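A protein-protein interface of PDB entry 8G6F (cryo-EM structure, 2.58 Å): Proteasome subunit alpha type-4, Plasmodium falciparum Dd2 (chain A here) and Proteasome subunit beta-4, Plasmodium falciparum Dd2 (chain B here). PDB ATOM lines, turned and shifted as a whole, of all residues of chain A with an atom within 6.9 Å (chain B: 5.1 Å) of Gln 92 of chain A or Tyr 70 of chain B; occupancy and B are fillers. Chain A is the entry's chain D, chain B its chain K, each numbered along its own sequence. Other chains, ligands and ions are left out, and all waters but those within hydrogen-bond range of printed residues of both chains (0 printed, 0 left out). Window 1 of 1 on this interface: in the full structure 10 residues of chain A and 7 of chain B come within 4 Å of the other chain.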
ATOM      1  N   LYS A  64      19.952 -19.958  -3.862  1.00  0.00           N
ATOM      2  CA  LYS A  64      19.745 -18.676  -3.206  1.00  0.00           C
ATOM      3  C   LYS A  64      19.548 -18.899  -1.715  1.00  0.00           C
ATOM      4  O   LYS A  64      18.705 -19.704  -1.311  1.00  0.00           O
ATOM      5  CB  LYS A  64      18.537 -17.946  -3.795  1.00  0.00           C
ATOM      6  CG  LYS A  64      18.597 -16.450  -3.611  1.00  0.00           C
ATOM      7  CD  LYS A  64      17.531 -15.735  -4.415  1.00  0.00           C
ATOM      8  CE  LYS A  64      17.542 -14.240  -4.137  1.00  0.00           C
ATOM      9  NZ  LYS A  64      18.912 -13.661  -4.227  1.00  0.00           N
ATOM     10  N   LEU A  65      20.321 -18.185  -0.900  1.00  0.00           N
ATOM     11  CA  LEU A  65      20.256 -18.346   0.545  1.00  0.00           C
ATOM     12  C   LEU A  65      19.186 -17.464   1.171  1.00  0.00           C
ATOM     13  O   LEU A  65      18.428 -17.924   2.030  1.00  0.00           O
ATOM     14  CB  LEU A  65      21.616 -18.025   1.163  1.00  0.00           C
ATOM     15  CG  LEU A  65      22.773 -18.840   0.596  1.00  0.00           C
ATOM     16  CD1 LEU A  65      24.086 -18.133   0.845  1.00  0.00           C
ATOM     17  CD2 LEU A  65      22.778 -20.230   1.196  1.00  0.00           C
ATOM     18  N   ASP A  66      19.120 -16.205   0.765  1.00  0.00           N
ATOM     19  CA  ASP A  66      18.085 -15.289   1.217  1.00  0.00           C
ATOM     20  C   ASP A  66      17.833 -14.307   0.079  1.00  0.00           C
ATOM     21  O   ASP A  66      18.200 -14.570  -1.070  1.00  0.00           O
ATOM     22  CB  ASP A  66      18.490 -14.618   2.541  1.00  0.00           C
ATOM     23  CG  ASP A  66      19.741 -13.772   2.417  1.00  0.00           C
ATOM     24  OD1 ASP A  66      19.822 -12.947   1.484  1.00  0.00           O
ATOM     25  OD2 ASP A  66      20.644 -13.924   3.264  1.00  0.00           O
ATOM     26  N   GLU A  67      17.198 -13.178   0.388  1.00  0.00           N
ATOM     27  CA  GLU A  67      16.815 -12.240  -0.660  1.00  0.00           C
ATOM     28  C   GLU A  67      18.004 -11.599  -1.365  1.00  0.00           C
ATOM     29  O   GLU A  67      17.809 -11.006  -2.430  1.00  0.00           O
ATOM     30  CB  GLU A  67      15.914 -11.139  -0.093  1.00  0.00           C
ATOM     31  CG  GLU A  67      16.320 -10.600   1.269  1.00  0.00           C
ATOM     32  CD  GLU A  67      15.359 -11.019   2.368  1.00  0.00           C
ATOM     33  OE1 GLU A  67      15.472 -12.164   2.857  1.00  0.00           O
ATOM     34  OE2 GLU A  67      14.485 -10.206   2.736  1.00  0.00           O
ATOM     35  N   HIS A  68      19.219 -11.699  -0.821  1.00  0.00           N
ATOM     36  CA  HIS A  68      20.357 -11.024  -1.437  1.00  0.00           C
ATOM     37  C   HIS A  68      21.624 -11.854  -1.552  1.00  0.00           C
ATOM     38  O   HIS A  68      22.562 -11.392  -2.206  1.00  0.00           O
ATOM     39  CB  HIS A  68      20.688  -9.742  -0.664  1.00  0.00           C
ATOM     40  CG  HIS A  68      19.575  -8.746  -0.654  1.00  0.00           C
ATOM     41  ND1 HIS A  68      19.089  -8.184   0.506  1.00  0.00           N
ATOM     42  CD2 HIS A  68      18.843  -8.220  -1.663  1.00  0.00           C
ATOM     43  CE1 HIS A  68      18.108  -7.351   0.211  1.00  0.00           C
ATOM     44  NE2 HIS A  68      17.939  -7.354  -1.098  1.00  0.00           N
ATOM     45  N   ASN A  85      21.299 -25.714   3.745  1.00  0.00           N
ATOM     46  CA  ASN A  85      20.149 -25.572   4.632  1.00  0.00           C
ATOM     47  C   ASN A  85      20.552 -24.923   5.948  1.00  0.00           C
ATOM     48  O   ASN A  85      19.841 -24.049   6.465  1.00  0.00           O
ATOM     49  CB  ASN A  85      19.497 -26.929   4.872  1.00  0.00           C
ATOM     50  CG  ASN A  85      18.595 -27.349   3.731  1.00  0.00           C
ATOM     51  OD1 ASN A  85      18.405 -26.605   2.770  1.00  0.00           O
ATOM     52  ND2 ASN A  85      18.039 -28.548   3.829  1.00  0.00           N
ATOM     53  N   THR A  87      22.951 -22.801   6.288  1.00  0.00           N
ATOM     54  CA  THR A  87      23.226 -21.400   5.997  1.00  0.00           C
ATOM     55  C   THR A  87      21.941 -20.599   5.826  1.00  0.00           C
ATOM     56  O   THR A  87      21.861 -19.451   6.268  1.00  0.00           O
ATOM     57  CB  THR A  87      24.098 -21.291   4.748  1.00  0.00           C
ATOM     58  OG1 THR A  87      25.274 -22.087   4.921  1.00  0.00           O
ATOM     59  CG2 THR A  87      24.503 -19.852   4.500  1.00  0.00           C
ATOM     60  N   ARG A  88      20.935 -21.172   5.166  1.00  0.00           N
ATOM     61  CA  ARG A  88      19.657 -20.481   5.032  1.00  0.00           C
ATOM     62  C   ARG A  88      19.016 -20.252   6.393  1.00  0.00           C
ATOM     63  O   ARG A  88      18.490 -19.162   6.677  1.00  0.00           O
ATOM     64  CB  ARG A  88      18.716 -21.287   4.141  1.00  0.00           C
ATOM     65  CG  ARG A  88      19.103 -21.325   2.688  1.00  0.00           C
ATOM     66  CD  ARG A  88      18.289 -22.360   1.953  1.00  0.00           C
ATOM     67  NE  ARG A  88      18.377 -22.202   0.508  1.00  0.00           N
ATOM     68  CZ  ARG A  88      18.205 -23.182  -0.366  1.00  0.00           C
ATOM     69  NH1 ARG A  88      17.934 -24.415   0.023  1.00  0.00           N
ATOM     70  NH2 ARG A  88      18.311 -22.918  -1.663  1.00  0.00           N
ATOM     71  N   LEU A  89      19.049 -21.271   7.252  1.00  0.00           N
ATOM     72  CA  LEU A  89      18.510 -21.098   8.592  1.00  0.00           C
ATOM     73  C   LEU A  89      19.252 -19.996   9.330  1.00  0.00           C
ATOM     74  O   LEU A  89      18.640 -19.199  10.046  1.00  0.00           O
ATOM     75  CB  LEU A  89      18.590 -22.413   9.362  1.00  0.00           C
ATOM     76  CG  LEU A  89      18.009 -22.366  10.774  1.00  0.00           C
ATOM     77  CD1 LEU A  89      16.916 -23.400  10.922  1.00  0.00           C
ATOM     78  CD2 LEU A  89      19.092 -22.585  11.803  1.00  0.00           C
ATOM     79  N   GLU A  90      20.574 -19.928   9.165  1.00  0.00           N
ATOM     80  CA  GLU A  90      21.340 -18.879   9.827  1.00  0.00           C
ATOM     81  C   GLU A  90      21.034 -17.500   9.252  1.00  0.00           C
ATOM     82  O   GLU A  90      21.042 -16.513   9.988  1.00  0.00           O
ATOM     83  CB  GLU A  90      22.833 -19.174   9.720  1.00  0.00           C
ATOM     84  CG  GLU A  90      23.706 -18.206  10.489  1.00  0.00           C
ATOM     85  CD  GLU A  90      23.263 -18.030  11.927  1.00  0.00           C
ATOM     86  OE1 GLU A  90      22.992 -19.047  12.595  1.00  0.00           O
ATOM     87  OE2 GLU A  90      23.186 -16.875  12.392  1.00  0.00           O
ATOM     88  N   CYS A  91      20.779 -17.406   7.949  1.00  0.00           N
ATOM     89  CA  CYS A  91      20.347 -16.138   7.371  1.00  0.00           C
ATOM     90  C   CYS A  91      19.077 -15.648   8.048  1.00  0.00           C
ATOM     91  O   CYS A  91      18.982 -14.487   8.466  1.00  0.00           O
ATOM     92  CB  CYS A  91      20.110 -16.293   5.869  1.00  0.00           C
ATOM     93  SG  CYS A  91      21.583 -16.331   4.845  1.00  0.00           S
ATOM     94  N   GLN A  92      18.085 -16.530   8.172  1.00  0.00           N
ATOM     95  CA  GLN A  92      16.836 -16.110   8.799  1.00  0.00           C
ATOM     96  C   GLN A  92      17.014 -15.840  10.289  1.00  0.00           C
ATOM     97  O   GLN A  92      16.351 -14.955  10.836  1.00  0.00           O
ATOM     98  CB  GLN A  92      15.745 -17.155   8.573  1.00  0.00           C
ATOM     99  CG  GLN A  92      15.161 -17.190   7.163  1.00  0.00           C
ATOM    100  CD  GLN A  92      15.099 -15.836   6.488  1.00  0.00           C
ATOM    101  OE1 GLN A  92      14.364 -14.951   6.915  1.00  0.00           O
ATOM    102  NE2 GLN A  92      15.871 -15.669   5.427  1.00  0.00           N
ATOM    103  N   ARG A  93      17.896 -16.580  10.961  1.00  0.00           N
ATOM    104  CA  ARG A  93      18.163 -16.317  12.371  1.00  0.00           C
ATOM    105  C   ARG A  93      18.809 -14.953  12.565  1.00  0.00           C
ATOM    106  O   ARG A  93      18.463 -14.220  13.498  1.00  0.00           O
ATOM    107  CB  ARG A  93      19.052 -17.415  12.945  1.00  0.00           C
ATOM    108  CG  ARG A  93      19.074 -17.469  14.459  1.00  0.00           C
ATOM    109  CD  ARG A  93      20.262 -18.261  14.976  1.00  0.00           C
ATOM    110  NE  ARG A  93      19.905 -19.645  15.277  1.00  0.00           N
ATOM    111  CZ  ARG A  93      20.324 -20.708  14.601  1.00  0.00           C
ATOM    112  NH1 ARG A  93      21.120 -20.599  13.550  1.00  0.00           N
ATOM    113  NH2 ARG A  93      19.929 -21.918  14.990  1.00  0.00           N
ATOM    114  N   TYR A  94      19.755 -14.598  11.698  1.00  0.00           N
ATOM    115  CA  TYR A  94      20.347 -13.268  11.755  1.00  0.00           C
ATOM    116  C   TYR A  94      19.296 -12.199  11.510  1.00  0.00           C
ATOM    117  O   TYR A  94      19.274 -11.172  12.195  1.00  0.00           O
ATOM    118  CB  TYR A  94      21.475 -13.157  10.730  1.00  0.00           C
ATOM    119  CG  TYR A  94      22.197 -11.832  10.734  1.00  0.00           C
ATOM    120  CD1 TYR A  94      21.631 -10.708  10.152  1.00  0.00           C
ATOM    121  CD2 TYR A  94      23.449 -11.704  11.311  1.00  0.00           C
ATOM    122  CE1 TYR A  94      22.284  -9.499  10.155  1.00  0.00           C
ATOM    123  CE2 TYR A  94      24.110 -10.495  11.316  1.00  0.00           C
ATOM    124  CZ  TYR A  94      23.524  -9.399  10.733  1.00  0.00           C
ATOM    125  OH  TYR A  94      24.177  -8.193  10.733  1.00  0.00           O
ATOM    126  N   TYR A  95      18.422 -12.413  10.527  1.00  0.00           N
ATOM    127  CA  TYR A  95      17.369 -11.436  10.277  1.00  0.00           C
ATOM    128  C   TYR A  95      16.480 -11.275  11.501  1.00  0.00           C
ATOM    129  O   TYR A  95      16.145 -10.155  11.893  1.00  0.00           O
ATOM    130  CB  TYR A  95      16.543 -11.852   9.064  1.00  0.00           C
ATOM    131  CG  TYR A  95      15.921 -10.701   8.309  1.00  0.00           C
ATOM    132  CD1 TYR A  95      15.583  -9.522   8.950  1.00  0.00           C
ATOM    133  CD2 TYR A  95      15.663 -10.800   6.955  1.00  0.00           C
ATOM    134  CE1 TYR A  95      15.017  -8.479   8.268  1.00  0.00           C
ATOM    135  CE2 TYR A  95      15.097  -9.756   6.264  1.00  0.00           C
ATOM    136  CZ  TYR A  95      14.777  -8.600   6.926  1.00  0.00           C
ATOM    137  OH  TYR A  95      14.208  -7.559   6.236  1.00  0.00           O
ATOM    138  N   LEU A  96      16.107 -12.384  12.135  1.00  0.00           N
ATOM    139  CA  LEU A  96      15.264 -12.309  13.320  1.00  0.00           C
ATOM    140  C   LEU A  96      15.965 -11.579  14.460  1.00  0.00           C
ATOM    141  O   LEU A  96      15.335 -10.810  15.194  1.00  0.00           O
ATOM    142  CB  LEU A  96      14.861 -13.716  13.755  1.00  0.00           C
ATOM    143  CG  LEU A  96      13.716 -13.837  14.758  1.00  0.00           C
ATOM    144  CD1 LEU A  96      12.467 -13.145  14.258  1.00  0.00           C
ATOM    145  CD2 LEU A  96      13.434 -15.295  15.042  1.00  0.00           C
ATOM    146  N   ASN A  97      17.264 -11.810  14.632  1.00  0.00           N
ATOM    147  CA  ASN A  97      17.973 -11.265  15.782  1.00  0.00           C
ATOM    148  C   ASN A  97      18.424  -9.824  15.595  1.00  0.00           C
ATOM    149  O   ASN A  97      18.639  -9.129  16.592  1.00  0.00           O
ATOM    150  CB  ASN A  97      19.188 -12.133  16.104  1.00  0.00           C
ATOM    151  CG  ASN A  97      18.833 -13.333  16.952  1.00  0.00           C
ATOM    152  OD1 ASN A  97      18.221 -13.200  18.010  1.00  0.00           O
ATOM    153  ND2 ASN A  97      19.207 -14.517  16.489  1.00  0.00           N
ATOM    154  N   ALA A 102      21.100 -10.592   6.542  1.00  0.00           N
ATOM    155  CA  ALA A 102      22.477 -10.984   6.813  1.00  0.00           C
ATOM    156  C   ALA A 102      23.366 -10.577   5.645  1.00  0.00           C
ATOM    157  O   ALA A 102      23.054 -10.908   4.496  1.00  0.00           O
ATOM    158  CB  ALA A 102      22.569 -12.486   7.048  1.00  0.00           C
ATOM    159  N   ILE A 107      27.738 -14.058   6.248  1.00  0.00           N
ATOM    160  CA  ILE A 107      27.314 -15.408   5.893  1.00  0.00           C
ATOM    161  C   ILE A 107      28.507 -16.258   5.476  1.00  0.00           C
ATOM    162  O   ILE A 107      28.592 -17.444   5.818  1.00  0.00           O
ATOM    163  CB  ILE A 107      26.227 -15.356   4.803  1.00  0.00           C
ATOM    164  CG1 ILE A 107      24.846 -15.262   5.451  1.00  0.00           C
ATOM    165  CG2 ILE A 107      26.286 -16.573   3.901  1.00  0.00           C
ATOM    166  CD1 ILE A 107      24.421 -16.517   6.219  1.00  0.00           C
ATOM    167  N   HIS B  40       6.407 -12.642   1.392  1.00  0.00           N
ATOM    168  CA  HIS B  40       6.606 -12.879  -0.028  1.00  0.00           C
ATOM    169  C   HIS B  40       5.637 -13.936  -0.526  1.00  0.00           C
ATOM    170  O   HIS B  40       5.276 -14.863   0.203  1.00  0.00           O
ATOM    171  CB  HIS B  40       8.041 -13.335  -0.303  1.00  0.00           C
ATOM    172  CG  HIS B  40       9.094 -12.452   0.289  1.00  0.00           C
ATOM    173  ND1 HIS B  40       8.956 -11.085   0.385  1.00  0.00           N
ATOM    174  CD2 HIS B  40      10.312 -12.743   0.802  1.00  0.00           C
ATOM    175  CE1 HIS B  40      10.040 -10.573   0.939  1.00  0.00           C
ATOM    176  NE2 HIS B  40      10.878 -11.558   1.201  1.00  0.00           N
ATOM    177  N   LYS B  63       9.740 -15.032   9.489  1.00  0.00           N
ATOM    178  CA  LYS B  63      11.038 -15.637   9.222  1.00  0.00           C
ATOM    179  C   LYS B  63      10.903 -17.126   8.962  1.00  0.00           C
ATOM    180  O   LYS B  63      11.604 -17.671   8.106  1.00  0.00           O
ATOM    181  CB  LYS B  63      12.001 -15.389  10.382  1.00  0.00           C
ATOM    182  CG  LYS B  63      12.291 -13.930  10.697  1.00  0.00           C
ATOM    183  CD  LYS B  63      12.631 -13.098   9.484  1.00  0.00           C
ATOM    184  CE  LYS B  63      12.643 -11.627   9.837  1.00  0.00           C
ATOM    185  NZ  LYS B  63      11.519 -10.898   9.203  1.00  0.00           N
ATOM    186  N   VAL B  65       8.281 -18.638   7.582  1.00  0.00           N
ATOM    187  CA  VAL B  65       7.703 -18.812   6.254  1.00  0.00           C
ATOM    188  C   VAL B  65       8.727 -18.485   5.175  1.00  0.00           C
ATOM    189  O   VAL B  65       8.811 -19.174   4.153  1.00  0.00           O
ATOM    190  CB  VAL B  65       6.429 -17.960   6.106  1.00  0.00           C
ATOM    191  CG1 VAL B  65       5.942 -17.980   4.673  1.00  0.00           C
ATOM    192  CG2 VAL B  65       5.347 -18.465   7.036  1.00  0.00           C
ATOM    193  N   HIS B  66       9.519 -17.430   5.376  1.00  0.00           N
ATOM    194  CA  HIS B  66      10.556 -17.100   4.406  1.00  0.00           C
ATOM    195  C   HIS B  66      11.606 -18.197   4.335  1.00  0.00           C
ATOM    196  O   HIS B  66      12.102 -18.520   3.252  1.00  0.00           O
ATOM    197  CB  HIS B  66      11.200 -15.759   4.757  1.00  0.00           C
ATOM    198  CG  HIS B  66      10.344 -14.575   4.433  1.00  0.00           C
ATOM    199  ND1 HIS B  66      10.708 -13.285   4.749  1.00  0.00           N
ATOM    200  CD2 HIS B  66       9.138 -14.486   3.828  1.00  0.00           C
ATOM    201  CE1 HIS B  66       9.764 -12.453   4.350  1.00  0.00           C
ATOM    202  NE2 HIS B  66       8.800 -13.157   3.788  1.00  0.00           N
ATOM    203  N   LEU B  67      11.961 -18.784   5.478  1.00  0.00           N
ATOM    204  CA  LEU B  67      12.881 -19.913   5.469  1.00  0.00           C
ATOM    205  C   LEU B  67      12.305 -21.080   4.682  1.00  0.00           C
ATOM    206  O   LEU B  67      13.016 -21.722   3.906  1.00  0.00           O
ATOM    207  CB  LEU B  67      13.189 -20.345   6.898  1.00  0.00           C
ATOM    208  CG  LEU B  67      14.154 -21.518   7.043  1.00  0.00           C
ATOM    209  CD1 LEU B  67      15.471 -21.222   6.363  1.00  0.00           C
ATOM    210  CD2 LEU B  67      14.362 -21.845   8.499  1.00  0.00           C
ATOM    211  N   TYR B  68      11.022 -21.379   4.882  1.00  0.00           N
ATOM    212  CA  TYR B  68      10.395 -22.456   4.126  1.00  0.00           C
ATOM    213  C   TYR B  68      10.478 -22.181   2.632  1.00  0.00           C
ATOM    214  O   TYR B  68      10.859 -23.055   1.842  1.00  0.00           O
ATOM    215  CB  TYR B  68       8.937 -22.616   4.563  1.00  0.00           C
ATOM    216  CG  TYR B  68       8.131 -23.564   3.703  1.00  0.00           C
ATOM    217  CD1 TYR B  68       7.580 -23.147   2.500  1.00  0.00           C
ATOM    218  CD2 TYR B  68       7.915 -24.873   4.098  1.00  0.00           C
ATOM    219  CE1 TYR B  68       6.852 -24.007   1.718  1.00  0.00           C
ATOM    220  CE2 TYR B  68       7.183 -25.738   3.320  1.00  0.00           C
ATOM    221  CZ  TYR B  68       6.656 -25.301   2.134  1.00  0.00           C
ATOM    222  OH  TYR B  68       5.926 -26.163   1.356  1.00  0.00           O
ATOM    223  N   GLN B  69      10.132 -20.961   2.230  1.00  0.00           N
ATOM    224  CA  GLN B  69      10.095 -20.628   0.813  1.00  0.00           C
ATOM    225  C   GLN B  69      11.485 -20.630   0.196  1.00  0.00           C
ATOM    226  O   GLN B  69      11.642 -21.026  -0.961  1.00  0.00           O
ATOM    227  CB  GLN B  69       9.412 -19.278   0.625  1.00  0.00           C
ATOM    228  CG  GLN B  69       7.951 -19.308   1.023  1.00  0.00           C
ATOM    229  CD  GLN B  69       7.235 -18.004   0.776  1.00  0.00           C
ATOM    230  OE1 GLN B  69       6.108 -17.996   0.294  1.00  0.00           O
ATOM    231  NE2 GLN B  69       7.874 -16.897   1.116  1.00  0.00           N
ATOM    232  N   TYR B  70      12.505 -20.209   0.943  1.00  0.00           N
ATOM    233  CA  TYR B  70      13.865 -20.265   0.416  1.00  0.00           C
ATOM    234  C   TYR B  70      14.364 -21.700   0.323  1.00  0.00           C
ATOM    235  O   TYR B  70      14.974 -22.083  -0.679  1.00  0.00           O
ATOM    236  CB  TYR B  70      14.803 -19.428   1.284  1.00  0.00           C
ATOM    237  CG  TYR B  70      14.613 -17.943   1.108  1.00  0.00           C
ATOM    238  CD1 TYR B  70      14.603 -17.373  -0.153  1.00  0.00           C
ATOM    239  CD2 TYR B  70      14.440 -17.112   2.202  1.00  0.00           C
ATOM    240  CE1 TYR B  70      14.421 -16.025  -0.321  1.00  0.00           C
ATOM    241  CE2 TYR B  70      14.261 -15.759   2.043  1.00  0.00           C
ATOM    242  CZ  TYR B  70      14.251 -15.223   0.779  1.00  0.00           C
ATOM    243  OH  TYR B  70      14.073 -13.874   0.609  1.00  0.00           O
ATOM    244  N   GLN B  71      14.100 -22.513   1.348  1.00  0.00           N
ATOM    245  CA  GLN B  71      14.569 -23.893   1.335  1.00  0.00           C
ATOM    246  C   GLN B  71      13.920 -24.689   0.215  1.00  0.00           C
ATOM    247  O   GLN B  71      14.565 -25.545  -0.397  1.00  0.00           O
ATOM    248  CB  GLN B  71      14.289 -24.554   2.682  1.00  0.00           C
ATOM    249  CG  GLN B  71      15.448 -24.485   3.648  1.00  0.00           C
ATOM    250  CD  GLN B  71      15.062 -24.903   5.047  1.00  0.00           C
ATOM    251  OE1 GLN B  71      13.882 -25.024   5.364  1.00  0.00           O
ATOM    252  NE2 GLN B  71      16.058 -25.122   5.895  1.00  0.00           N
ATOM    253  N   ASN B  72      12.646 -24.435  -0.062  1.00  0.00           N
ATOM    254  CA  ASN B  72      11.909 -25.221  -1.038  1.00  0.00           C
ATOM    255  C   ASN B  72      11.770 -24.532  -2.387  1.00  0.00           C
ATOM    256  O   ASN B  72      11.146 -25.094  -3.288  1.00  0.00           O
ATOM    257  CB  ASN B  72      10.526 -25.561  -0.479  1.00  0.00           C
ATOM    258  CG  ASN B  72      10.605 -26.282   0.847  1.00  0.00           C
ATOM    259  OD1 ASN B  72      10.127 -25.789   1.862  1.00  0.00           O
ATOM    260  ND2 ASN B  72      11.227 -27.449   0.846  1.00  0.00           N
ATOM    261  N   ASN B  73      12.339 -23.340  -2.552  1.00  0.00           N
ATOM    262  CA  ASN B  73      12.300 -22.633  -3.829  1.00  0.00           C
ATOM    263  C   ASN B  73      10.874 -22.555  -4.363  1.00  0.00           C
ATOM    264  O   ASN B  73      10.615 -22.790  -5.542  1.00  0.00           O
ATOM    265  CB  ASN B  73      13.226 -23.294  -4.848  1.00  0.00           C
ATOM    266  CG  ASN B  73      13.554 -22.382  -6.012  1.00  0.00           C
ATOM    267  OD1 ASN B  73      13.516 -21.159  -5.888  1.00  0.00           O
ATOM    268  ND2 ASN B  73      13.880 -22.973  -7.152  1.00  0.00           N
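The side-chain hydroxyl (OH) of Tyr 70 of chain B is in hydrogen-bond range of the side-chain carboxylate (OE1) of Glu 67 of chain A (3.2 Å).
The side-chain amino group (NZ) of Lys 64 of chain A lies close to the backbone carbonyl oxygen (O) of Asp 66 of chain A. The backbone NH of His 40 of chain B lies close to a ring nitrogen (NE2) of His 66 of chain B, at 3.4 Å. OD1 of Asp 66 of chain A sits at hydrogen-bond distance from N of His 68 of chain A (2.7 Å). O of Lys 64 of chain A is in hydrogen-bond range of NE of Arg 88 of chain A, 3.1 Å away. The side-chain carboxylate (OD2) of Asp 66 of chain A sits at hydrogen-bond distance from the side-chain sulfur (SG) of Cys 91 of chain A, at 3.0 Å. The side-chain amino group (NZ) of Lys 64 of chain A is in hydrogen-bond range of the backbone carbonyl oxygen (O) of Glu 67 of chain A, 3.4 Å away.
Among the printed residues, merely in contact across the chains: Arg 88 of chain A with Tyr 70 of chain B (3.4 Å), Arg 88 of chain A with Gln 71 of chain B (3.6 Å), Gln 92 of chain A with Lys 63 of chain B (3.6 Å), Leu 96 of chain A with Lys 63 of chain B (3.7 Å), Arg 88 of chain A with Leu 67 of chain B (3.7 Å), Leu 89 of chain A with Leu 67 of chain B (3.7 Å), Tyr 95 of chain A with Lys 63 of chain B (3.7 Å), Gln 92 of chain A with Leu 67 of chain B (3.7 Å), Asn 85 of chain A with Gln 71 of chain B (3.7 Å), Gln 92 of chain A with Tyr 70 of chain B (3.7 Å), Asp 66 of chain A with Tyr 70 of chain B (3.8 Å), Gln 92 of chain A with His 66 of chain B (3.9 Å) and Leu 65 of chain A with Tyr 70 of chain B (3.9 Å).
Gln 92 of chain A touches just these residues of chain B: Lys 63 (3.6 Å), His 66 (3.9 Å), Leu 67 (3.7 Å) and Tyr 70 (3.7 Å). Tyr 70 of chain B touches just these residues of chain A: Leu 65 (3.9 Å), Asp 66 (3.8 Å), Glu 67 (3.2 Å), Arg 88 (3.4 Å) and Gln 92 (3.7 Å). Printed residues of chain A within 4 Å of Leu 67 of chain B: Arg 88 (3.7 Å), Leu 89 (3.7 Å) and Gln 92 (3.7 Å). Printed residues of chain A within 4 Å of Lys 63 of chain B: Gln 92 (3.6 Å), Tyr 95 (3.7 Å) and Leu 96 (3.7 Å). Of the printed residues of chain B, Leu 96 of chain A touches Lys 63. Thr 87 of chain A touches none of the printed residues of chain B. Gln 69 of chain B touches none of the printed residues of chain A. The nearest printed residue of chain B that does not touch Gln 92 of chain A is Tyr 68 of chain B (6.3 Å).
Printed residues of chain A that touch a printed residue of chain B: Leu 65, Asp 66, Glu 67, Asn 85, Arg 88, Leu 89, Gln 92, Tyr 95 and Leu 96. Hydrophobic or aromatic side chains of chain A within 4 Å of the printed part of chain B: Leu 89, Tyr 95 and Leu 96. Of the 11 printed residues of chain B, 5 touch a printed residue of chain A. Hydrophobic or aromatic side chains of chain B that line the printed part of chain A: His 66, Leu 67 and Tyr 70. Among the printed residues, 14 pairs touch across the chains.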
